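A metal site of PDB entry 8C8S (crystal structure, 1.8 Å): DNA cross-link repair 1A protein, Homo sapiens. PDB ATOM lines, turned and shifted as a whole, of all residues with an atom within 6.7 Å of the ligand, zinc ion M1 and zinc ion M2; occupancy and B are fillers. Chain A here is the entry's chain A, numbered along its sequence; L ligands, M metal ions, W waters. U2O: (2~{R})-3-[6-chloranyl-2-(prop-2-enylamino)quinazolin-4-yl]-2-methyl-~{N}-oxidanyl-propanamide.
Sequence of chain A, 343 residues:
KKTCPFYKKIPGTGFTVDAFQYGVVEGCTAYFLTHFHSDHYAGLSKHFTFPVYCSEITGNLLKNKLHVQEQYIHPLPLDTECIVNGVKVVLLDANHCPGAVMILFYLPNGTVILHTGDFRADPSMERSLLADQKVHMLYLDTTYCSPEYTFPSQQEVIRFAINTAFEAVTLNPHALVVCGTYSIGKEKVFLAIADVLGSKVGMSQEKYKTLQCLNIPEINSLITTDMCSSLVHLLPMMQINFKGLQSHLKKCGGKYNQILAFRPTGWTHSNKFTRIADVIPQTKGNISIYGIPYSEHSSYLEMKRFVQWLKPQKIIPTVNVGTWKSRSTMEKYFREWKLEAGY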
ATOM      1  N   HIS A  35     -26.650 -17.405  30.989  1.00  0.00           N
ATOM      2  CA  HIS A  35     -25.190 -17.528  31.020  1.00  0.00           C
ATOM      3  C   HIS A  35     -24.576 -16.327  31.705  1.00  0.00           C
ATOM      4  O   HIS A  35     -25.215 -15.298  31.908  1.00  0.00           O
ATOM      5  CB  HIS A  35     -24.592 -17.689  29.624  1.00  0.00           C
ATOM      6  CG  HIS A  35     -24.824 -16.522  28.719  1.00  0.00           C
ATOM      7  ND1 HIS A  35     -26.076 -16.188  28.243  1.00  0.00           N
ATOM      8  CD2 HIS A  35     -23.967 -15.625  28.192  1.00  0.00           C
ATOM      9  CE1 HIS A  35     -25.968 -15.134  27.446  1.00  0.00           C
ATOM     10  NE2 HIS A  35     -24.694 -14.774  27.411  1.00  0.00           N
ATOM     11  N   PHE A  36     -23.275 -16.450  32.010  1.00  0.00           N
ATOM     12  CA  PHE A  36     -22.592 -15.456  32.838  1.00  0.00           C
ATOM     13  C   PHE A  36     -21.871 -14.417  31.961  1.00  0.00           C
ATOM     14  O   PHE A  36     -20.644 -14.331  31.899  1.00  0.00           O
ATOM     15  CB  PHE A  36     -21.633 -16.154  33.797  1.00  0.00           C
ATOM     16  CG  PHE A  36     -21.096 -15.248  34.880  1.00  0.00           C
ATOM     17  CD1 PHE A  36     -21.894 -14.871  35.943  1.00  0.00           C
ATOM     18  CD2 PHE A  36     -19.774 -14.802  34.829  1.00  0.00           C
ATOM     19  CE1 PHE A  36     -21.386 -14.029  36.955  1.00  0.00           C
ATOM     20  CE2 PHE A  36     -19.267 -13.959  35.841  1.00  0.00           C
ATOM     21  CZ  PHE A  36     -20.071 -13.582  36.896  1.00  0.00           C
ATOM     22  N   HIS A  37     -22.671 -13.623  31.255  1.00  0.00           N
ATOM     23  CA  HIS A  37     -22.177 -12.435  30.565  1.00  0.00           C
ATOM     24  C   HIS A  37     -22.886 -11.212  31.142  1.00  0.00           C
ATOM     25  O   HIS A  37     -24.084 -11.281  31.449  1.00  0.00           O
ATOM     26  CB  HIS A  37     -22.404 -12.507  29.052  1.00  0.00           C
ATOM     27  CG  HIS A  37     -21.359 -13.320  28.330  1.00  0.00           C
ATOM     28  ND1 HIS A  37     -21.570 -13.854  27.080  1.00  0.00           N
ATOM     29  CD2 HIS A  37     -20.103 -13.665  28.675  1.00  0.00           C
ATOM     30  CE1 HIS A  37     -20.495 -14.501  26.690  1.00  0.00           C
ATOM     31  NE2 HIS A  37     -19.584 -14.401  27.642  1.00  0.00           N
ATOM     32  N   SER A  38     -22.165 -10.103  31.257  1.00  0.00           N
ATOM     33  CA  SER A  38     -22.650  -8.965  32.046  1.00  0.00           C
ATOM     34  C   SER A  38     -23.934  -8.371  31.505  1.00  0.00           C
ATOM     35  O   SER A  38     -24.775  -7.896  32.281  1.00  0.00           O
ATOM     36  CB  SER A  38     -21.570  -7.891  32.160  1.00  0.00           C
ATOM     37  OG  SER A  38     -21.111  -7.482  30.884  1.00  0.00           O
ATOM     38  N   ASP A  39     -24.141  -8.368  30.186  1.00  0.00           N
ATOM     39  CA  ASP A  39     -25.407  -7.840  29.687  1.00  0.00           C
ATOM     40  C   ASP A  39     -26.610  -8.676  30.106  1.00  0.00           C
ATOM     41  O   ASP A  39     -27.750  -8.210  29.961  1.00  0.00           O
ATOM     42  CB  ASP A  39     -25.371  -7.678  28.158  1.00  0.00           C
ATOM     43  CG  ASP A  39     -24.660  -8.819  27.435  1.00  0.00           C
ATOM     44  OD1 ASP A  39     -23.613  -9.294  27.942  1.00  0.00           O
ATOM     45  OD2 ASP A  39     -25.142  -9.243  26.339  1.00  0.00           O
ATOM     46  N   HIS A  40     -26.396  -9.884  30.656  1.00  0.00           N
ATOM     47  CA  HIS A  40     -27.470 -10.762  31.085  1.00  0.00           C
ATOM     48  C   HIS A  40     -27.626 -10.858  32.587  1.00  0.00           C
ATOM     49  O   HIS A  40     -28.750 -10.950  33.087  1.00  0.00           O
ATOM     50  CB  HIS A  40     -27.266 -12.153  30.502  1.00  0.00           C
ATOM     51  CG  HIS A  40     -27.249 -12.159  29.010  1.00  0.00           C
ATOM     52  ND1 HIS A  40     -28.306 -12.612  28.251  1.00  0.00           N
ATOM     53  CD2 HIS A  40     -26.326 -11.702  28.128  1.00  0.00           C
ATOM     54  CE1 HIS A  40     -28.034 -12.448  26.970  1.00  0.00           C
ATOM     55  NE2 HIS A  40     -26.840 -11.893  26.875  1.00  0.00           N
ATOM     56  N   HIS A  96     -22.467 -21.374  23.294  1.00  0.00           N
ATOM     57  CA  HIS A  96     -22.076 -19.975  23.409  1.00  0.00           C
ATOM     58  C   HIS A  96     -20.768 -19.915  24.206  1.00  0.00           C
ATOM     59  O   HIS A  96     -19.732 -20.367  23.711  1.00  0.00           O
ATOM     60  CB  HIS A  96     -23.209 -19.178  24.059  1.00  0.00           C
ATOM     61  CG  HIS A  96     -23.002 -17.708  24.082  1.00  0.00           C
ATOM     62  ND1 HIS A  96     -22.640 -16.985  22.971  1.00  0.00           N
ATOM     63  CD2 HIS A  96     -23.161 -16.800  25.081  1.00  0.00           C
ATOM     64  CE1 HIS A  96     -22.549 -15.706  23.281  1.00  0.00           C
ATOM     65  NE2 HIS A  96     -22.850 -15.578  24.559  1.00  0.00           N
ATOM     66  N   CYS A  97     -20.801 -19.425  25.424  1.00  0.00           N
ATOM     67  CA  CYS A  97     -19.654 -19.474  26.334  1.00  0.00           C
ATOM     68  C   CYS A  97     -19.822 -20.613  27.334  1.00  0.00           C
ATOM     69  O   CYS A  97     -20.880 -21.236  27.408  1.00  0.00           O
ATOM     70  CB  CYS A  97     -19.522 -18.139  27.047  1.00  0.00           C
ATOM     71  SG  CYS A  97     -20.925 -17.836  28.112  1.00  0.00           S
ATOM     72  N   ALA A 100     -23.295 -21.672  29.235  1.00  0.00           N
ATOM     73  CA  ALA A 100     -24.429 -21.030  28.570  1.00  0.00           C
ATOM     74  C   ALA A 100     -25.469 -22.069  28.164  1.00  0.00           C
ATOM     75  O   ALA A 100     -25.119 -23.122  27.637  1.00  0.00           O
ATOM     76  CB  ALA A 100     -23.932 -20.251  27.349  1.00  0.00           C
ATOM     77  N   GLY A 117     -31.417 -18.077  24.920  1.00  0.00           N
ATOM     78  CA  GLY A 117     -30.400 -17.230  25.517  1.00  0.00           C
ATOM     79  C   GLY A 117     -29.550 -16.653  24.398  1.00  0.00           C
ATOM     80  O   GLY A 117     -30.061 -16.303  23.331  1.00  0.00           O
ATOM     81  N   ASP A 118     -28.239 -16.599  24.610  1.00  0.00           N
ATOM     82  CA  ASP A 118     -27.313 -16.404  23.500  1.00  0.00           C
ATOM     83  C   ASP A 118     -26.852 -17.779  23.011  1.00  0.00           C
ATOM     84  O   ASP A 118     -26.498 -18.649  23.812  1.00  0.00           O
ATOM     85  CB  ASP A 118     -26.076 -15.616  23.923  1.00  0.00           C
ATOM     86  CG  ASP A 118     -26.333 -14.126  24.139  1.00  0.00           C
ATOM     87  OD1 ASP A 118     -27.427 -13.606  23.850  1.00  0.00           O
ATOM     88  OD2 ASP A 118     -25.379 -13.506  24.599  1.00  0.00           O
ATOM     89  N   ASP A 141     -32.082 -15.503  19.873  1.00  0.00           N
ATOM     90  CA  ASP A 141     -30.880 -14.658  19.809  1.00  0.00           C
ATOM     91  C   ASP A 141     -30.660 -14.272  18.361  1.00  0.00           C
ATOM     92  O   ASP A 141     -30.121 -15.050  17.562  1.00  0.00           O
ATOM     93  CB  ASP A 141     -29.671 -15.404  20.382  1.00  0.00           C
ATOM     94  CG  ASP A 141     -28.336 -14.699  20.090  1.00  0.00           C
ATOM     95  OD1 ASP A 141     -28.317 -13.486  19.767  1.00  0.00           O
ATOM     96  OD2 ASP A 141     -27.287 -15.379  20.198  1.00  0.00           O
ATOM     97  N   THR A 143     -28.694 -11.776  17.202  1.00  0.00           N
ATOM     98  CA  THR A 143     -27.571 -10.838  17.156  1.00  0.00           C
ATOM     99  C   THR A 143     -27.132 -10.559  15.720  1.00  0.00           C
ATOM    100  O   THR A 143     -26.924  -9.395  15.335  1.00  0.00           O
ATOM    101  CB  THR A 143     -26.399 -11.399  17.976  1.00  0.00           C
ATOM    102  OG1 THR A 143     -26.825 -11.565  19.337  1.00  0.00           O
ATOM    103  CG2 THR A 143     -25.173 -10.459  17.966  1.00  0.00           C
ATOM    104  N   TYR A 144     -27.014 -11.598  14.905  1.00  0.00           N
ATOM    105  CA  TYR A 144     -26.526 -11.518  13.539  1.00  0.00           C
ATOM    106  C   TYR A 144     -27.593 -11.937  12.539  1.00  0.00           C
ATOM    107  O   TYR A 144     -27.320 -12.659  11.570  1.00  0.00           O
ATOM    108  CB  TYR A 144     -25.260 -12.368  13.389  1.00  0.00           C
ATOM    109  CG  TYR A 144     -24.078 -11.814  14.137  1.00  0.00           C
ATOM    110  CD1 TYR A 144     -23.699 -10.496  13.964  1.00  0.00           C
ATOM    111  CD2 TYR A 144     -23.353 -12.597  15.015  1.00  0.00           C
ATOM    112  CE1 TYR A 144     -22.615  -9.959  14.645  1.00  0.00           C
ATOM    113  CE2 TYR A 144     -22.261 -12.081  15.701  1.00  0.00           C
ATOM    114  CZ  TYR A 144     -21.901 -10.761  15.504  1.00  0.00           C
ATOM    115  OH  TYR A 144     -20.844 -10.226  16.182  1.00  0.00           O
ATOM    116  N   TYR A 182     -12.201 -10.259  27.528  1.00  0.00           N
ATOM    117  CA  TYR A 182     -13.091  -9.290  28.158  1.00  0.00           C
ATOM    118  C   TYR A 182     -14.055  -9.916  29.146  1.00  0.00           C
ATOM    119  O   TYR A 182     -14.514  -9.221  30.065  1.00  0.00           O
ATOM    120  CB  TYR A 182     -13.894  -8.524  27.087  1.00  0.00           C
ATOM    121  N   SER A 183     -14.376 -11.183  28.988  1.00  0.00           N
ATOM    122  CA  SER A 183     -15.348 -11.897  29.809  1.00  0.00           C
ATOM    123  C   SER A 183     -15.162 -13.377  29.484  1.00  0.00           C
ATOM    124  O   SER A 183     -14.221 -13.755  28.779  1.00  0.00           O
ATOM    125  CB  SER A 183     -16.781 -11.416  29.549  1.00  0.00           C
ATOM    126  OG  SER A 183     -17.140 -11.560  28.194  1.00  0.00           O
ATOM    127  N   ILE A 184     -16.035 -14.233  30.001  1.00  0.00           N
ATOM    128  CA  ILE A 184     -15.868 -15.644  29.684  1.00  0.00           C
ATOM    129  C   ILE A 184     -16.294 -15.891  28.233  1.00  0.00           C
ATOM    130  O   ILE A 184     -16.961 -15.066  27.593  1.00  0.00           O
ATOM    131  CB  ILE A 184     -16.635 -16.567  30.645  1.00  0.00           C
ATOM    132  CG1 ILE A 184     -18.141 -16.336  30.546  1.00  0.00           C
ATOM    133  CG2 ILE A 184     -16.126 -16.384  32.091  1.00  0.00           C
ATOM    134  CD1 ILE A 184     -18.948 -17.437  31.243  1.00  0.00           C
ATOM    135  N   LYS A 186     -14.715 -17.985  24.434  1.00  0.00           N
ATOM    136  CA  LYS A 186     -13.607 -17.901  23.490  1.00  0.00           C
ATOM    137  C   LYS A 186     -12.294 -18.381  24.096  1.00  0.00           C
ATOM    138  O   LYS A 186     -11.225 -18.060  23.595  1.00  0.00           O
ATOM    139  CB  LYS A 186     -13.475 -16.467  22.949  1.00  0.00           C
ATOM    140  CG  LYS A 186     -14.829 -15.884  22.447  1.00  0.00           C
ATOM    141  CD  LYS A 186     -14.689 -14.572  21.636  1.00  0.00           C
ATOM    142  CE  LYS A 186     -16.059 -14.008  21.259  1.00  0.00           C
ATOM    143  NZ  LYS A 186     -15.930 -12.805  20.357  1.00  0.00           N
ATOM    144  N   GLY A 266     -16.059 -10.224  17.287  1.00  0.00           N
ATOM    145  CA  GLY A 266     -17.166 -10.863  16.602  1.00  0.00           C
ATOM    146  C   GLY A 266     -17.064 -10.602  15.119  1.00  0.00           C
ATOM    147  O   GLY A 266     -15.969 -10.582  14.545  1.00  0.00           O
ATOM    148  N   TRP A 267     -18.206 -10.398  14.471  1.00  0.00           N
ATOM    149  CA  TRP A 267     -18.223  -9.984  13.068  1.00  0.00           C
ATOM    150  C   TRP A 267     -17.629  -8.592  12.913  1.00  0.00           C
ATOM    151  O   TRP A 267     -17.836  -7.716  13.757  1.00  0.00           O
ATOM    152  CB  TRP A 267     -19.655 -10.010  12.534  1.00  0.00           C
ATOM    153  CG  TRP A 267     -19.803  -9.435  11.145  1.00  0.00           C
ATOM    154  CD1 TRP A 267     -19.695 -10.118   9.965  1.00  0.00           C
ATOM    155  CD2 TRP A 267     -20.089  -8.080  10.803  1.00  0.00           C
ATOM    156  NE1 TRP A 267     -19.884  -9.261   8.910  1.00  0.00           N
ATOM    157  CE2 TRP A 267     -20.138  -8.002   9.395  1.00  0.00           C
ATOM    158  CE3 TRP A 267     -20.311  -6.916  11.544  1.00  0.00           C
ATOM    159  CZ2 TRP A 267     -20.397  -6.808   8.714  1.00  0.00           C
ATOM    160  CZ3 TRP A 267     -20.577  -5.724  10.870  1.00  0.00           C
ATOM    161  CH2 TRP A 267     -20.617  -5.686   9.463  1.00  0.00           C
ATOM    162  N   GLU A 296     -19.200 -16.537  19.045  1.00  0.00           N
ATOM    163  CA  GLU A 296     -20.029 -17.439  19.829  1.00  0.00           C
ATOM    164  C   GLU A 296     -21.502 -17.115  19.661  1.00  0.00           C
ATOM    165  O   GLU A 296     -22.340 -17.526  20.482  1.00  0.00           O
ATOM    166  CB  GLU A 296     -19.594 -17.418  21.304  1.00  0.00           C
ATOM    167  CG  GLU A 296     -18.172 -18.033  21.434  1.00  0.00           C
ATOM    168  CD  GLU A 296     -17.691 -18.277  22.875  1.00  0.00           C
ATOM    169  OE1 GLU A 296     -18.108 -17.538  23.792  1.00  0.00           O
ATOM    170  OE2 GLU A 296     -16.883 -19.220  23.069  1.00  0.00           O
ATOM    171  N   HIS A 297     -21.840 -16.388  18.595  1.00  0.00           N
ATOM    172  CA  HIS A 297     -23.206 -16.216  18.129  1.00  0.00           C
ATOM    173  C   HIS A 297     -23.373 -16.808  16.739  1.00  0.00           C
ATOM    174  O   HIS A 297     -22.435 -16.805  15.919  1.00  0.00           O
ATOM    175  CB  HIS A 297     -23.604 -14.718  18.076  1.00  0.00           C
ATOM    176  CG  HIS A 297     -23.705 -14.047  19.414  1.00  0.00           C
ATOM    177  ND1 HIS A 297     -24.835 -14.119  20.198  1.00  0.00           N
ATOM    178  CD2 HIS A 297     -22.825 -13.260  20.085  1.00  0.00           C
ATOM    179  CE1 HIS A 297     -24.647 -13.424  21.303  1.00  0.00           C
ATOM    180  NE2 HIS A 297     -23.439 -12.886  21.258  1.00  0.00           N
ATOM    181  N   VAL A 319     -32.672  -9.661  20.505  1.00  0.00           N
ATOM    182  CA  VAL A 319     -31.538  -8.787  20.205  1.00  0.00           C
ATOM    183  C   VAL A 319     -31.905  -7.930  18.997  1.00  0.00           C
ATOM    184  O   VAL A 319     -32.636  -8.360  18.104  1.00  0.00           O
ATOM    185  CB  VAL A 319     -30.240  -9.605  19.920  1.00  0.00           C
ATOM    186  CG1 VAL A 319     -29.034  -8.666  19.698  1.00  0.00           C
ATOM    187  CG2 VAL A 319     -29.939 -10.596  21.042  1.00  0.00           C
HETATM  188  C1  U2O L   1     -19.270 -11.623  25.109  1.00  0.00           C
HETATM  189  C10 U2O L   1     -22.805  -6.457  24.618  1.00  0.00           C
HETATM  190  C11 U2O L   1     -22.633  -7.917  22.814  1.00  0.00           C
HETATM  191  C12 U2O L   1     -22.452  -9.393  20.851  1.00  0.00           C
HETATM  192  C13 U2O L   1     -21.841  -9.091  19.550  1.00  0.00           C
HETATM  193  C14 U2O L   1     -21.797  -7.930  18.962  1.00  0.00           C
HETATM  194  C15 U2O L   1     -21.772 -11.621  24.907  1.00  0.00           C
HETATM  195  C2  U2O L   1     -20.495 -10.808  24.682  1.00  0.00           C
HETATM  196  C3  U2O L   1     -20.563  -9.463  25.435  1.00  0.00           C
HETATM  197  C4  U2O L   1     -21.466  -8.485  24.737  1.00  0.00           C
HETATM  198  C5  U2O L   1     -21.960  -7.296  25.373  1.00  0.00           C
HETATM  199  C6  U2O L   1     -21.628  -6.935  26.692  1.00  0.00           C
HETATM  200  C7  U2O L   1     -22.134  -5.782  27.221  1.00  0.00           C
HETATM  201  C8  U2O L   1     -22.981  -4.935  26.481  1.00  0.00           C
HETATM  202  C9  U2O L   1     -23.313  -5.271  25.202  1.00  0.00           C
HETATM  203  N1  U2O L   1     -23.135  -6.781  23.326  1.00  0.00           N
HETATM  204  N2  U2O L   1     -22.969  -8.225  21.553  1.00  0.00           N
HETATM  205  N3  U2O L   1     -21.809  -8.773  23.471  1.00  0.00           N
HETATM  206  N4  U2O L   1     -22.598 -11.175  25.832  1.00  0.00           N
HETATM  207  O1  U2O L   1     -23.799 -11.833  26.077  1.00  0.00           O
HETATM  208  O2  U2O L   1     -22.018 -12.614  24.224  1.00  0.00           O
HETATM  209 CL1  U2O L   1     -21.736  -5.330  28.851  1.00  0.00          CL
HETATM  210 ZN    ZN M   1     -23.406 -13.820  25.787  1.00  0.00          ZN
HETATM  211 ZN    ZN M   2     -25.541 -11.376  25.129  1.00  0.00          ZN
HETATM  212  O   HOH W   1     -24.155 -10.906  23.538  1.00  0.00           O
HETATM  213  O   HOH W   2     -27.313 -11.184  23.826  1.00  0.00           O
HETATM  214  O   HOH W   3     -20.084 -13.298  22.413  1.00  0.00           O
HETATM  215  O   HOH W   4     -20.026  -9.515  28.594  1.00  0.00           O
HETATM  216  O   HOH W   5     -25.985  -9.958  21.464  1.00  0.00           O
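An oxygen (O2) of the ligand lies close to a ring nitrogen (NE2) of His 297 (3.3 Å).
O of Glu 296 lies within hydrogen-bond range of ND1 of His 96. A ring nitrogen (NE2) of His 37 sits at hydrogen-bond distance from the backbone carbonyl oxygen (O) of Ile 184 (2.7 Å). SG of Cys 97 lies close to NE2 of His 37. ND1 of His 297 lies within hydrogen-bond range of OG1 of Thr 143. The side-chain carboxylate (OD2) of Asp 141 lies within hydrogen-bond range of a ring nitrogen (ND1) of His 297 (2.8 Å). The backbone NH (N) of Trp 267 is in hydrogen-bond range of the side-chain hydroxyl (OH) of Tyr 144 (3.1 Å). OD1 of Asp 141 sits at hydrogen-bond distance from OG1 of Thr 143 (2.5 Å).
Merely in contact with the ligand: Ser 38 (3.0 Å), Thr 143 (3.9 Å), Tyr 144 (3.7 Å) and Ser 183 (3.7 Å). 11 residues have an atom within 4 Å of the ligand: His 35, His 37, Ser 38, Asp 39, His 40, His 96, Asp 118, Thr 143, Tyr 144, Ser 183 and His 297. The nearest printed residue that does not touch the ligand is Ile 184 (4.8 Å).
Within 4 Å of zinc ion M1: His 35, His 37, His 96 and Asp 118.
Of the 23 residues printed, 3 come within 4 Å of zinc ion M2. The nearest printed residue that does not touch zinc ion M2 is His 35 (4.2 Å).
Zinc ion M1 is bound by O1 of the ligand (2.0 Å), NE2 of His 96 (2.2 Å), ND1 of His 37 (2.2 Å), NE2 of His 35 (2.3 Å), OD2 of Asp 118 (2.3 Å) and O2 of the ligand (2.4 Å).
Zinc ion M2 is bound by an oxygen (O1) of the ligand (2.0 Å), water W1 (2.2 Å), the side-chain carboxylate of Asp 118 (2.2 Å), water W2 (2.2 Å), a ring nitrogen (NE2) of His 40 (2.2 Å) and the side-chain carboxylate of Asp 39 (2.5 Å). Zinc ion M2 has six donor atoms within binding distance.
Water W1 lies within hydrogen-bond range of N4 of the ligand (2.8 Å) and NE2 of His 297 (3.1 Å). Water W5 bridges the side-chain hydroxyl of Thr 143 (2.8 Å) and a nitrogen (N2) of the ligand (3.5 Å).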
